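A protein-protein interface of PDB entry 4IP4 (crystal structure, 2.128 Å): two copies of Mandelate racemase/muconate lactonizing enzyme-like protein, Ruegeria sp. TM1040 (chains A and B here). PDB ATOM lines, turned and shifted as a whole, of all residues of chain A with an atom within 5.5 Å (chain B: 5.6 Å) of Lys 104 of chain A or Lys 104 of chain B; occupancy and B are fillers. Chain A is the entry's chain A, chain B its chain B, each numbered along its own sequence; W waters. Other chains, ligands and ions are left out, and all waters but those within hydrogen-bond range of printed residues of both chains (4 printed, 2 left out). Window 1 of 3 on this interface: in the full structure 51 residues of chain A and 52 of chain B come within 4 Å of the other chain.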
ATOM      1  N   ILE A 100      -9.042   8.197   1.881  1.00  0.00           N
ATOM      2  CA  ILE A 100      -8.709   6.786   2.106  1.00  0.00           C
ATOM      3  C   ILE A 100      -7.474   6.652   3.008  1.00  0.00           C
ATOM      4  O   ILE A 100      -7.179   5.580   3.530  1.00  0.00           O
ATOM      5  CB  ILE A 100      -8.461   6.089   0.741  1.00  0.00           C
ATOM      6  CG1 ILE A 100      -9.589   6.443  -0.234  1.00  0.00           C
ATOM      7  CG2 ILE A 100      -8.340   4.580   0.881  1.00  0.00           C
ATOM      8  CD1 ILE A 100     -10.986   6.131   0.301  1.00  0.00           C
ATOM      9  N   GLY A 101      -6.747   7.757   3.171  1.00  0.00           N
ATOM     10  CA  GLY A 101      -5.602   7.825   4.062  1.00  0.00           C
ATOM     11  C   GLY A 101      -5.933   8.737   5.238  1.00  0.00           C
ATOM     12  O   GLY A 101      -6.676   8.332   6.133  1.00  0.00           O
ATOM     13  N   PRO A 102      -5.386   9.972   5.249  1.00  0.00           N
ATOM     14  CA  PRO A 102      -4.436  10.503   4.258  1.00  0.00           C
ATOM     15  C   PRO A 102      -2.998  10.114   4.580  1.00  0.00           C
ATOM     16  O   PRO A 102      -2.625  10.079   5.756  1.00  0.00           O
ATOM     17  CB  PRO A 102      -4.588  12.034   4.392  1.00  0.00           C
ATOM     18  CG  PRO A 102      -5.783  12.250   5.366  1.00  0.00           C
ATOM     19  CD  PRO A 102      -5.805  11.010   6.205  1.00  0.00           C
ATOM     20  N   ASP A 103      -2.202   9.851   3.543  1.00  0.00           N
ATOM     21  CA  ASP A 103      -0.798   9.482   3.718  1.00  0.00           C
ATOM     22  C   ASP A 103      -0.605   8.354   4.744  1.00  0.00           C
ATOM     23  O   ASP A 103       0.229   8.453   5.644  1.00  0.00           O
ATOM     24  CB  ASP A 103       0.057  10.701   4.107  1.00  0.00           C
ATOM     25  CG  ASP A 103       0.114  11.759   3.012  1.00  0.00           C
ATOM     26  OD1 ASP A 103      -0.435  11.528   1.906  1.00  0.00           O
ATOM     27  OD2 ASP A 103       0.722  12.825   3.262  1.00  0.00           O
ATOM     28  N   LYS A 104      -1.382   7.284   4.604  1.00  0.00           N
ATOM     29  CA  LYS A 104      -1.226   6.103   5.447  1.00  0.00           C
ATOM     30  C   LYS A 104      -1.960   4.937   4.801  1.00  0.00           C
ATOM     31  O   LYS A 104      -2.825   5.147   3.946  1.00  0.00           O
ATOM     32  CB  LYS A 104      -1.792   6.356   6.843  1.00  0.00           C
ATOM     33  CG  LYS A 104      -3.319   6.413   6.863  1.00  0.00           C
ATOM     34  CD  LYS A 104      -3.851   6.955   8.188  1.00  0.00           C
ATOM     35  CE  LYS A 104      -3.533   8.440   8.371  1.00  0.00           C
ATOM     36  NZ  LYS A 104      -4.201   8.955   9.609  1.00  0.00           N
ATOM     37  N   GLY A 105      -1.626   3.710   5.196  1.00  0.00           N
ATOM     38  CA  GLY A 105      -2.357   2.549   4.697  1.00  0.00           C
ATOM     39  C   GLY A 105      -2.150   2.302   3.208  1.00  0.00           C
ATOM     40  O   GLY A 105      -1.161   2.752   2.626  1.00  0.00           O
ATOM     41  N   ALA A 106      -3.097   1.608   2.584  1.00  0.00           N
ATOM     42  CA  ALA A 106      -2.961   1.188   1.190  1.00  0.00           C
ATOM     43  C   ALA A 106      -2.642   2.317   0.200  1.00  0.00           C
ATOM     44  O   ALA A 106      -1.832   2.142  -0.719  1.00  0.00           O
ATOM     45  CB  ALA A 106      -4.207   0.441   0.746  1.00  0.00           C
ATOM     46  N   ILE A 107      -3.285   3.466   0.375  1.00  0.00           N
ATOM     47  CA  ILE A 107      -3.120   4.557  -0.579  1.00  0.00           C
ATOM     48  C   ILE A 107      -1.685   5.086  -0.538  1.00  0.00           C
ATOM     49  O   ILE A 107      -1.141   5.495  -1.564  1.00  0.00           O
ATOM     50  CB  ILE A 107      -4.156   5.702  -0.343  1.00  0.00           C
ATOM     51  CG1 ILE A 107      -4.226   6.626  -1.560  1.00  0.00           C
ATOM     52  CG2 ILE A 107      -3.833   6.488   0.931  1.00  0.00           C
ATOM     53  CD1 ILE A 107      -4.663   5.932  -2.854  1.00  0.00           C
ATOM     54  N   HIS A 108      -1.056   5.042   0.638  1.00  0.00           N
ATOM     55  CA  HIS A 108       0.297   5.576   0.772  1.00  0.00           C
ATOM     56  C   HIS A 108       1.372   4.557   0.360  1.00  0.00           C
ATOM     57  O   HIS A 108       2.350   4.921  -0.293  1.00  0.00           O
ATOM     58  CB  HIS A 108       0.553   6.152   2.174  1.00  0.00           C
ATOM     59  CG  HIS A 108       1.387   7.399   2.156  1.00  0.00           C
ATOM     60  ND1 HIS A 108       1.302   8.329   1.142  1.00  0.00           N
ATOM     61  CD2 HIS A 108       2.339   7.856   3.005  1.00  0.00           C
ATOM     62  CE1 HIS A 108       2.156   9.314   1.372  1.00  0.00           C
ATOM     63  NE2 HIS A 108       2.797   9.052   2.498  1.00  0.00           N
ATOM     64  N   LEU A 109       1.177   3.290   0.727  1.00  0.00           N
ATOM     65  CA  LEU A 109       1.966   2.200   0.156  1.00  0.00           C
ATOM     66  C   LEU A 109       1.990   2.325  -1.377  1.00  0.00           C
ATOM     67  O   LEU A 109       3.048   2.264  -2.008  1.00  0.00           O
ATOM     68  CB  LEU A 109       1.373   0.845   0.572  1.00  0.00           C
ATOM     69  CG  LEU A 109       1.505   0.486   2.058  1.00  0.00           C
ATOM     70  CD1 LEU A 109       0.570  -0.671   2.438  1.00  0.00           C
ATOM     71  CD2 LEU A 109       2.944   0.125   2.387  1.00  0.00           C
ATOM     72  N   PRO A 277       3.160   0.716  16.005  1.00  0.00           N
ATOM     73  CA  PRO A 277       3.975   1.708  15.295  1.00  0.00           C
ATOM     74  C   PRO A 277       3.373   3.110  15.331  1.00  0.00           C
ATOM     75  O   PRO A 277       3.996   4.037  14.823  1.00  0.00           O
ATOM     76  CB  PRO A 277       4.013   1.172  13.860  1.00  0.00           C
ATOM     77  CG  PRO A 277       2.752   0.382  13.722  1.00  0.00           C
ATOM     78  CD  PRO A 277       2.473  -0.208  15.085  1.00  0.00           C
ATOM     79  N   ASP A 278       2.189   3.258  15.922  1.00  0.00           N
ATOM     80  CA  ASP A 278       1.547   4.563  16.046  1.00  0.00           C
ATOM     81  C   ASP A 278       1.786   5.186  17.412  1.00  0.00           C
ATOM     82  O   ASP A 278       1.422   6.339  17.649  1.00  0.00           O
ATOM     83  CB  ASP A 278       0.030   4.445  15.852  1.00  0.00           C
ATOM     84  CG  ASP A 278      -0.349   3.886  14.495  1.00  0.00           C
ATOM     85  OD1 ASP A 278       0.470   3.982  13.543  1.00  0.00           O
ATOM     86  OD2 ASP A 278      -1.477   3.351  14.385  1.00  0.00           O
ATOM     87  N   MET A 300       6.995   0.604   9.804  1.00  0.00           N
ATOM     88  CA  MET A 300       5.596   0.838   9.487  1.00  0.00           C
ATOM     89  C   MET A 300       5.146   2.248   9.872  1.00  0.00           C
ATOM     90  O   MET A 300       3.946   2.535   9.889  1.00  0.00           O
ATOM     91  CB  MET A 300       4.690  -0.176  10.203  1.00  0.00           C
ATOM     92  CG  MET A 300       4.725  -1.577   9.641  1.00  0.00           C
ATOM     93  SD  MET A 300       3.190  -2.416  10.068  1.00  0.00           S
ATOM     94  CE  MET A 300       3.570  -4.068   9.510  1.00  0.00           C
ATOM     95  N   GLN A 302       3.850   5.573   9.387  1.00  0.00           N
ATOM     96  CA  GLN A 302       3.040   5.816   8.189  1.00  0.00           C
ATOM     97  C   GLN A 302       3.509   6.958   7.301  1.00  0.00           C
ATOM     98  O   GLN A 302       3.361   6.891   6.081  1.00  0.00           O
ATOM     99  CB  GLN A 302       1.566   6.018   8.568  1.00  0.00           C
ATOM    100  CG  GLN A 302       1.323   7.222   9.446  1.00  0.00           C
ATOM    101  CD  GLN A 302       0.056   7.069  10.292  1.00  0.00           C
ATOM    102  OE1 GLN A 302      -0.211   5.996  10.827  1.00  0.00           O
ATOM    103  NE2 GLN A 302      -0.722   8.139  10.401  1.00  0.00           N
ATOM    104  N   ASN A 303       4.080   7.998   7.903  1.00  0.00           N
ATOM    105  CA  ASN A 303       4.427   9.203   7.151  1.00  0.00           C
ATOM    106  C   ASN A 303       5.331  10.148   7.942  1.00  0.00           C
ATOM    107  O   ASN A 303       5.643   9.879   9.102  1.00  0.00           O
ATOM    108  CB  ASN A 303       3.148   9.931   6.682  1.00  0.00           C
ATOM    109  CG  ASN A 303       2.267  10.391   7.841  1.00  0.00           C
ATOM    110  OD1 ASN A 303       2.767  10.767   8.901  1.00  0.00           O
ATOM    111  ND2 ASN A 303       0.936  10.382   7.630  1.00  0.00           N
ATOM    112  N   ILE B 100      -1.117  -4.012   5.637  1.00  0.00           N
ATOM    113  CA  ILE B 100      -1.732  -2.982   4.803  1.00  0.00           C
ATOM    114  C   ILE B 100      -2.135  -1.776   5.664  1.00  0.00           C
ATOM    115  O   ILE B 100      -2.398  -0.689   5.148  1.00  0.00           O
ATOM    116  CB  ILE B 100      -2.967  -3.560   4.057  1.00  0.00           C
ATOM    117  CG1 ILE B 100      -2.624  -4.929   3.463  1.00  0.00           C
ATOM    118  CG2 ILE B 100      -3.434  -2.630   2.956  1.00  0.00           C
ATOM    119  CD1 ILE B 100      -1.460  -4.903   2.492  1.00  0.00           C
ATOM    120  N   GLY B 101      -2.181  -1.984   6.980  1.00  0.00           N
ATOM    121  CA  GLY B 101      -2.420  -0.914   7.938  1.00  0.00           C
ATOM    122  C   GLY B 101      -1.205  -0.612   8.812  1.00  0.00           C
ATOM    123  O   GLY B 101      -0.271   0.039   8.357  1.00  0.00           O
ATOM    124  N   PRO B 102      -1.212  -1.071  10.078  1.00  0.00           N
ATOM    125  CA  PRO B 102      -2.325  -1.753  10.757  1.00  0.00           C
ATOM    126  C   PRO B 102      -3.352  -0.759  11.297  1.00  0.00           C
ATOM    127  O   PRO B 102      -2.968   0.338  11.697  1.00  0.00           O
ATOM    128  CB  PRO B 102      -1.645  -2.474  11.934  1.00  0.00           C
ATOM    129  CG  PRO B 102      -0.128  -2.367  11.664  1.00  0.00           C
ATOM    130  CD  PRO B 102       0.014  -1.087  10.893  1.00  0.00           C
ATOM    131  N   ASP B 103      -4.624  -1.154  11.317  1.00  0.00           N
ATOM    132  CA  ASP B 103      -5.690  -0.343  11.908  1.00  0.00           C
ATOM    133  C   ASP B 103      -5.657   1.104  11.395  1.00  0.00           C
ATOM    134  O   ASP B 103      -5.739   2.054  12.168  1.00  0.00           O
ATOM    135  CB  ASP B 103      -5.636  -0.386  13.455  1.00  0.00           C
ATOM    136  CG  ASP B 103      -5.948  -1.772  14.029  1.00  0.00           C
ATOM    137  OD1 ASP B 103      -6.259  -2.689  13.253  1.00  0.00           O
ATOM    138  OD2 ASP B 103      -5.908  -1.951  15.270  1.00  0.00           O
ATOM    139  N   LYS B 104      -5.513   1.262  10.086  1.00  0.00           N
ATOM    140  CA  LYS B 104      -5.502   2.585   9.481  1.00  0.00           C
ATOM    141  C   LYS B 104      -5.738   2.479   7.979  1.00  0.00           C
ATOM    142  O   LYS B 104      -5.512   1.418   7.367  1.00  0.00           O
ATOM    143  CB  LYS B 104      -4.169   3.308   9.747  1.00  0.00           C
ATOM    144  CG  LYS B 104      -2.997   2.771   8.904  1.00  0.00           C
ATOM    145  CD  LYS B 104      -1.661   3.362   9.350  1.00  0.00           C
ATOM    146  CE  LYS B 104      -1.272   2.891  10.754  1.00  0.00           C
ATOM    147  NZ  LYS B 104       0.153   3.254  11.068  1.00  0.00           N
ATOM    148  N   GLY B 105      -6.188   3.582   7.387  1.00  0.00           N
ATOM    149  CA  GLY B 105      -6.425   3.630   5.955  1.00  0.00           C
ATOM    150  C   GLY B 105      -7.519   2.685   5.494  1.00  0.00           C
ATOM    151  O   GLY B 105      -8.440   2.350   6.258  1.00  0.00           O
ATOM    152  N   ALA B 106      -7.400   2.231   4.249  1.00  0.00           N
ATOM    153  CA  ALA B 106      -8.444   1.429   3.615  1.00  0.00           C
ATOM    154  C   ALA B 106      -8.817   0.156   4.382  1.00  0.00           C
ATOM    155  O   ALA B 106      -9.995  -0.208   4.435  1.00  0.00           O
ATOM    156  CB  ALA B 106      -8.069   1.099   2.160  1.00  0.00           C
ATOM    157  N   ILE B 107      -7.832  -0.525   4.968  1.00  0.00           N
ATOM    158  CA  ILE B 107      -8.123  -1.785   5.659  1.00  0.00           C
ATOM    159  C   ILE B 107      -8.937  -1.565   6.943  1.00  0.00           C
ATOM    160  O   ILE B 107      -9.720  -2.434   7.333  1.00  0.00           O
ATOM    161  CB  ILE B 107      -6.841  -2.633   5.940  1.00  0.00           C
ATOM    162  CG1 ILE B 107      -7.205  -4.089   6.282  1.00  0.00           C
ATOM    163  CG2 ILE B 107      -6.028  -2.037   7.079  1.00  0.00           C
ATOM    164  CD1 ILE B 107      -7.912  -4.854   5.155  1.00  0.00           C
ATOM    165  N   HIS B 108      -8.773  -0.408   7.590  1.00  0.00           N
ATOM    166  CA  HIS B 108      -9.516  -0.135   8.830  1.00  0.00           C
ATOM    167  C   HIS B 108     -10.885   0.473   8.532  1.00  0.00           C
ATOM    168  O   HIS B 108     -11.857   0.203   9.241  1.00  0.00           O
ATOM    169  CB  HIS B 108      -8.728   0.747   9.813  1.00  0.00           C
ATOM    170  CG  HIS B 108      -8.930   0.365  11.251  1.00  0.00           C
ATOM    171  ND1 HIS B 108      -9.094  -0.944  11.657  1.00  0.00           N
ATOM    172  CD2 HIS B 108      -8.996   1.116  12.378  1.00  0.00           C
ATOM    173  CE1 HIS B 108      -9.251  -0.982  12.970  1.00  0.00           C
ATOM    174  NE2 HIS B 108      -9.198   0.256  13.431  1.00  0.00           N
ATOM    175  N   LEU B 109     -10.958   1.281   7.477  1.00  0.00           N
ATOM    176  CA  LEU B 109     -12.252   1.746   6.975  1.00  0.00           C
ATOM    177  C   LEU B 109     -13.135   0.541   6.684  1.00  0.00           C
ATOM    178  O   LEU B 109     -14.306   0.504   7.060  1.00  0.00           O
ATOM    179  CB  LEU B 109     -12.070   2.597   5.715  1.00  0.00           C
ATOM    180  CG  LEU B 109     -11.433   3.970   5.947  1.00  0.00           C
ATOM    181  CD1 LEU B 109     -10.833   4.542   4.655  1.00  0.00           C
ATOM    182  CD2 LEU B 109     -12.472   4.907   6.503  1.00  0.00           C
ATOM    183  N   PRO B 277      -4.581  15.229  10.836  1.00  0.00           N
ATOM    184  CA  PRO B 277      -5.219  14.393  11.862  1.00  0.00           C
ATOM    185  C   PRO B 277      -4.222  13.456  12.573  1.00  0.00           C
ATOM    186  O   PRO B 277      -4.614  12.772  13.524  1.00  0.00           O
ATOM    187  CB  PRO B 277      -6.247  13.582  11.058  1.00  0.00           C
ATOM    188  CG  PRO B 277      -5.617  13.466   9.689  1.00  0.00           C
ATOM    189  CD  PRO B 277      -4.878  14.767   9.467  1.00  0.00           C
ATOM    190  N   ASP B 278      -2.964  13.427  12.123  1.00  0.00           N
ATOM    191  CA  ASP B 278      -1.935  12.603  12.764  1.00  0.00           C
ATOM    192  C   ASP B 278      -1.111  13.403  13.756  1.00  0.00           C
ATOM    193  O   ASP B 278      -0.308  12.847  14.511  1.00  0.00           O
ATOM    194  CB  ASP B 278      -0.982  12.026  11.717  1.00  0.00           C
ATOM    195  CG  ASP B 278      -1.684  11.125  10.735  1.00  0.00           C
ATOM    196  OD1 ASP B 278      -2.804  10.657  11.052  1.00  0.00           O
ATOM    197  OD2 ASP B 278      -1.114  10.884   9.651  1.00  0.00           O
ATOM    198  N   MET B 300     -10.967  11.888  11.274  1.00  0.00           N
ATOM    199  CA  MET B 300     -10.042  11.030  10.540  1.00  0.00           C
ATOM    200  C   MET B 300      -8.994  10.389  11.451  1.00  0.00           C
ATOM    201  O   MET B 300      -8.052   9.762  10.961  1.00  0.00           O
ATOM    202  CB  MET B 300      -9.330  11.802   9.421  1.00  0.00           C
ATOM    203  CG  MET B 300     -10.200  12.167   8.229  1.00  0.00           C
ATOM    204  SD  MET B 300      -9.153  12.277   6.776  1.00  0.00           S
ATOM    205  CE  MET B 300     -10.289  12.919   5.568  1.00  0.00           C
ATOM    206  N   GLN B 302      -7.161   7.784  13.164  1.00  0.00           N
ATOM    207  CA  GLN B 302      -7.205   6.466  12.536  1.00  0.00           C
ATOM    208  C   GLN B 302      -7.641   5.320  13.459  1.00  0.00           C
ATOM    209  O   GLN B 302      -8.252   4.356  13.001  1.00  0.00           O
ATOM    210  CB  GLN B 302      -5.852   6.142  11.899  1.00  0.00           C
ATOM    211  CG  GLN B 302      -4.722   6.014  12.912  1.00  0.00           C
ATOM    212  CD  GLN B 302      -3.360   6.296  12.295  1.00  0.00           C
ATOM    213  OE1 GLN B 302      -3.209   7.207  11.465  1.00  0.00           O
ATOM    214  NE2 GLN B 302      -2.364   5.527  12.699  1.00  0.00           N
ATOM    215  N   ASN B 303      -7.336   5.429  14.748  1.00  0.00           N
ATOM    216  CA  ASN B 303      -7.562   4.314  15.666  1.00  0.00           C
ATOM    217  C   ASN B 303      -7.452   4.725  17.127  1.00  0.00           C
ATOM    218  O   ASN B 303      -7.204   5.895  17.432  1.00  0.00           O
ATOM    219  CB  ASN B 303      -6.615   3.139  15.340  1.00  0.00           C
ATOM    220  CG  ASN B 303      -5.142   3.487  15.541  1.00  0.00           C
ATOM    221  OD1 ASN B 303      -4.784   4.258  16.437  1.00  0.00           O
ATOM    222  ND2 ASN B 303      -4.278   2.902  14.705  1.00  0.00           N
HETATM  223  O   HOH W   1      -6.990   8.510   8.890  1.00  0.00           O
HETATM  224  O   HOH W   2      -2.779  11.777   7.747  1.00  0.00           O
HETATM  225  O   HOH W   3      -1.027   0.953  13.734  1.00  0.00           O
HETATM  226  O   HOH W   4       1.481   2.011   8.992  1.00  0.00           O
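The backbone carbonyl oxygen of Ile 100 of chain A is in hydrogen-bond range of the backbone NH of Ala 106 of chain B.
The side-chain amino group of Lys 104 of chain A lies within salt-bridge range of the side-chain carboxylate of Asp 278 of chain B (2.6 Å).
NZ of Lys 104 of chain A is in hydrogen-bond range of OE1 of Gln 302 of chain B (2.7 Å).
OD1 of Asp 278 of chain A is in salt-bridge range of NZ of Lys 104 of chain B, at 2.6 Å.
NE2 of Gln 302 of chain B lies within hydrogen-bond range of OD2 of Asp 278 of chain A (2.9 Å).
The side-chain carboxylate (OD2) of Asp 278 of chain A lies within hydrogen-bond range of the side-chain amide nitrogen (ND2) of Asn 303 of chain B (2.9 Å).
OE1 of Gln 302 of chain A is in hydrogen-bond range of NZ of Lys 104 of chain B, 2.8 Å away.
The side-chain carboxylate (OD2) of Asp 278 of chain B lies within hydrogen-bond range of the side-chain amide nitrogen (NE2) of Gln 302 of chain A, at 2.9 Å.
The side-chain amide nitrogen of Gln 302 of chain A sits at hydrogen-bond distance from the side-chain amide oxygen of Gln 302 of chain B (2.9 Å).
The side-chain amide nitrogen of Asn 303 of chain A lies within hydrogen-bond range of the side-chain carboxylate of Asp 278 of chain B (2.9 Å).
Water W3 lies within hydrogen-bond range of OD2 of Asp 278 of chain A (2.5 Å) and O of Pro 102 of chain B (2.9 Å).
Water W2 lies within hydrogen-bond range of the backbone carbonyl oxygen of Pro 102 of chain A and the side-chain carboxylate of Asp 278 of chain B.
Water W1 lies within hydrogen-bond range of O of Met 300 of chain B (2.6 Å), O of Gly 101 of chain A (2.8 Å) and NZ of Lys 104 of chain A (2.9 Å).
Water W4 lies within hydrogen-bond range of O of Met 300 of chain A, O of Gly 101 of chain B and NZ of Lys 104 of chain B.
Ile 100 of chain A touches Gly 105 of chain B.
CD1 of Leu 109 of chain B touches O of Ile 100 of chain A, at 3.96 Å.
Pro 102 of chain A touches Met 300 of chain B (CD to SD, 3.6 Å).
CD of Lys 104 of chain B touches CB of Lys 104 of chain A (3.9 Å).
Gly 105 of chain A touches Ile 100 of chain B.
O of Ile 100 of chain B touches N of Ala 106 of chain A (3.5 Å).
SD of Met 300 of chain A touches CD of Pro 102 of chain B, at 3.5 Å.
Printed residues of chain B that touch a printed residue of chain A: Ile 100, Pro 102, Lys 104, Gly 105, Ala 106, Leu 109, Asp 278, Met 300, Gln 302 and Asn 303.
Hydrophobic or aromatic side chains of chain B within 4 Å of the printed part of chain A: Ile 100, Pro 102, Ala 106, Leu 109 and Met 300.
Of the 15 printed residues of chain A, 9 touch a printed residue of chain B.
Ile 100 of chain A touches Gly 105 of chain B, and with the chains exchanged Gly 105 of chain A touches Ile 100 of chain B.
Ile 100 of chain A touches Ala 106 of chain B, and with the chains exchanged Ala 106 of chain A touches Ile 100 of chain B.
Ile 100 of chain A touches Leu 109 of chain B, but with the chains exchanged Leu 109 of chain A does not touch Ile 100 of chain B (4.02 Å).
Asp 278 of chain A touches Gln 302 of chain B, and with the chains exchanged Gln 302 of chain A touches Asp 278 of chain B.
Of the 17 pairs that touch across the chains among the printed residues, 16 have their exchanged pair printed and touching as well.
Lys 104 of chain A touches three residues of chain B.
Printed residues of chain B within 4 Å of Asn 303 of chain A: Asp 278 (2.9 Å).
Of the printed residues of chain A, Ile 100 of chain B touches Gly 105 (3.3 Å) and Ala 106 (3.5 Å).
Of the printed residues of chain A, Pro 102 of chain B touches Met 300 (3.5 Å).
Of the printed residues of chain A, Lys 104 of chain B touches Lys 104, Asp 278 and Gln 302.
Printed residues of chain A within 4 Å of Ala 106 of chain B: Ile 100.
Of the printed residues of chain A, Asn 303 of chain B touches Asp 278 (2.9 Å).
The nearest residue of chain B that does not touch Lys 104 of chain A is Gly 105 of chain B (4.1 Å).
ND2 of Asn 303 of chain A is in hydrogen-bond range of O of Asp 103 of chain A (2.9 Å).
OD1 of Asp 278 of chain A lies close to OE1 of Gln 302 of chain A, 3.4 Å away.
The side-chain amide nitrogen (ND2) of Asn 303 of chain B lies within hydrogen-bond range of the backbone carbonyl oxygen (O) of Asp 103 of chain B (3.0 Å).
OD1 of Asp 278 of chain B sits close to OE1 of Gln 302 of chain B, at 3.5 Å.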
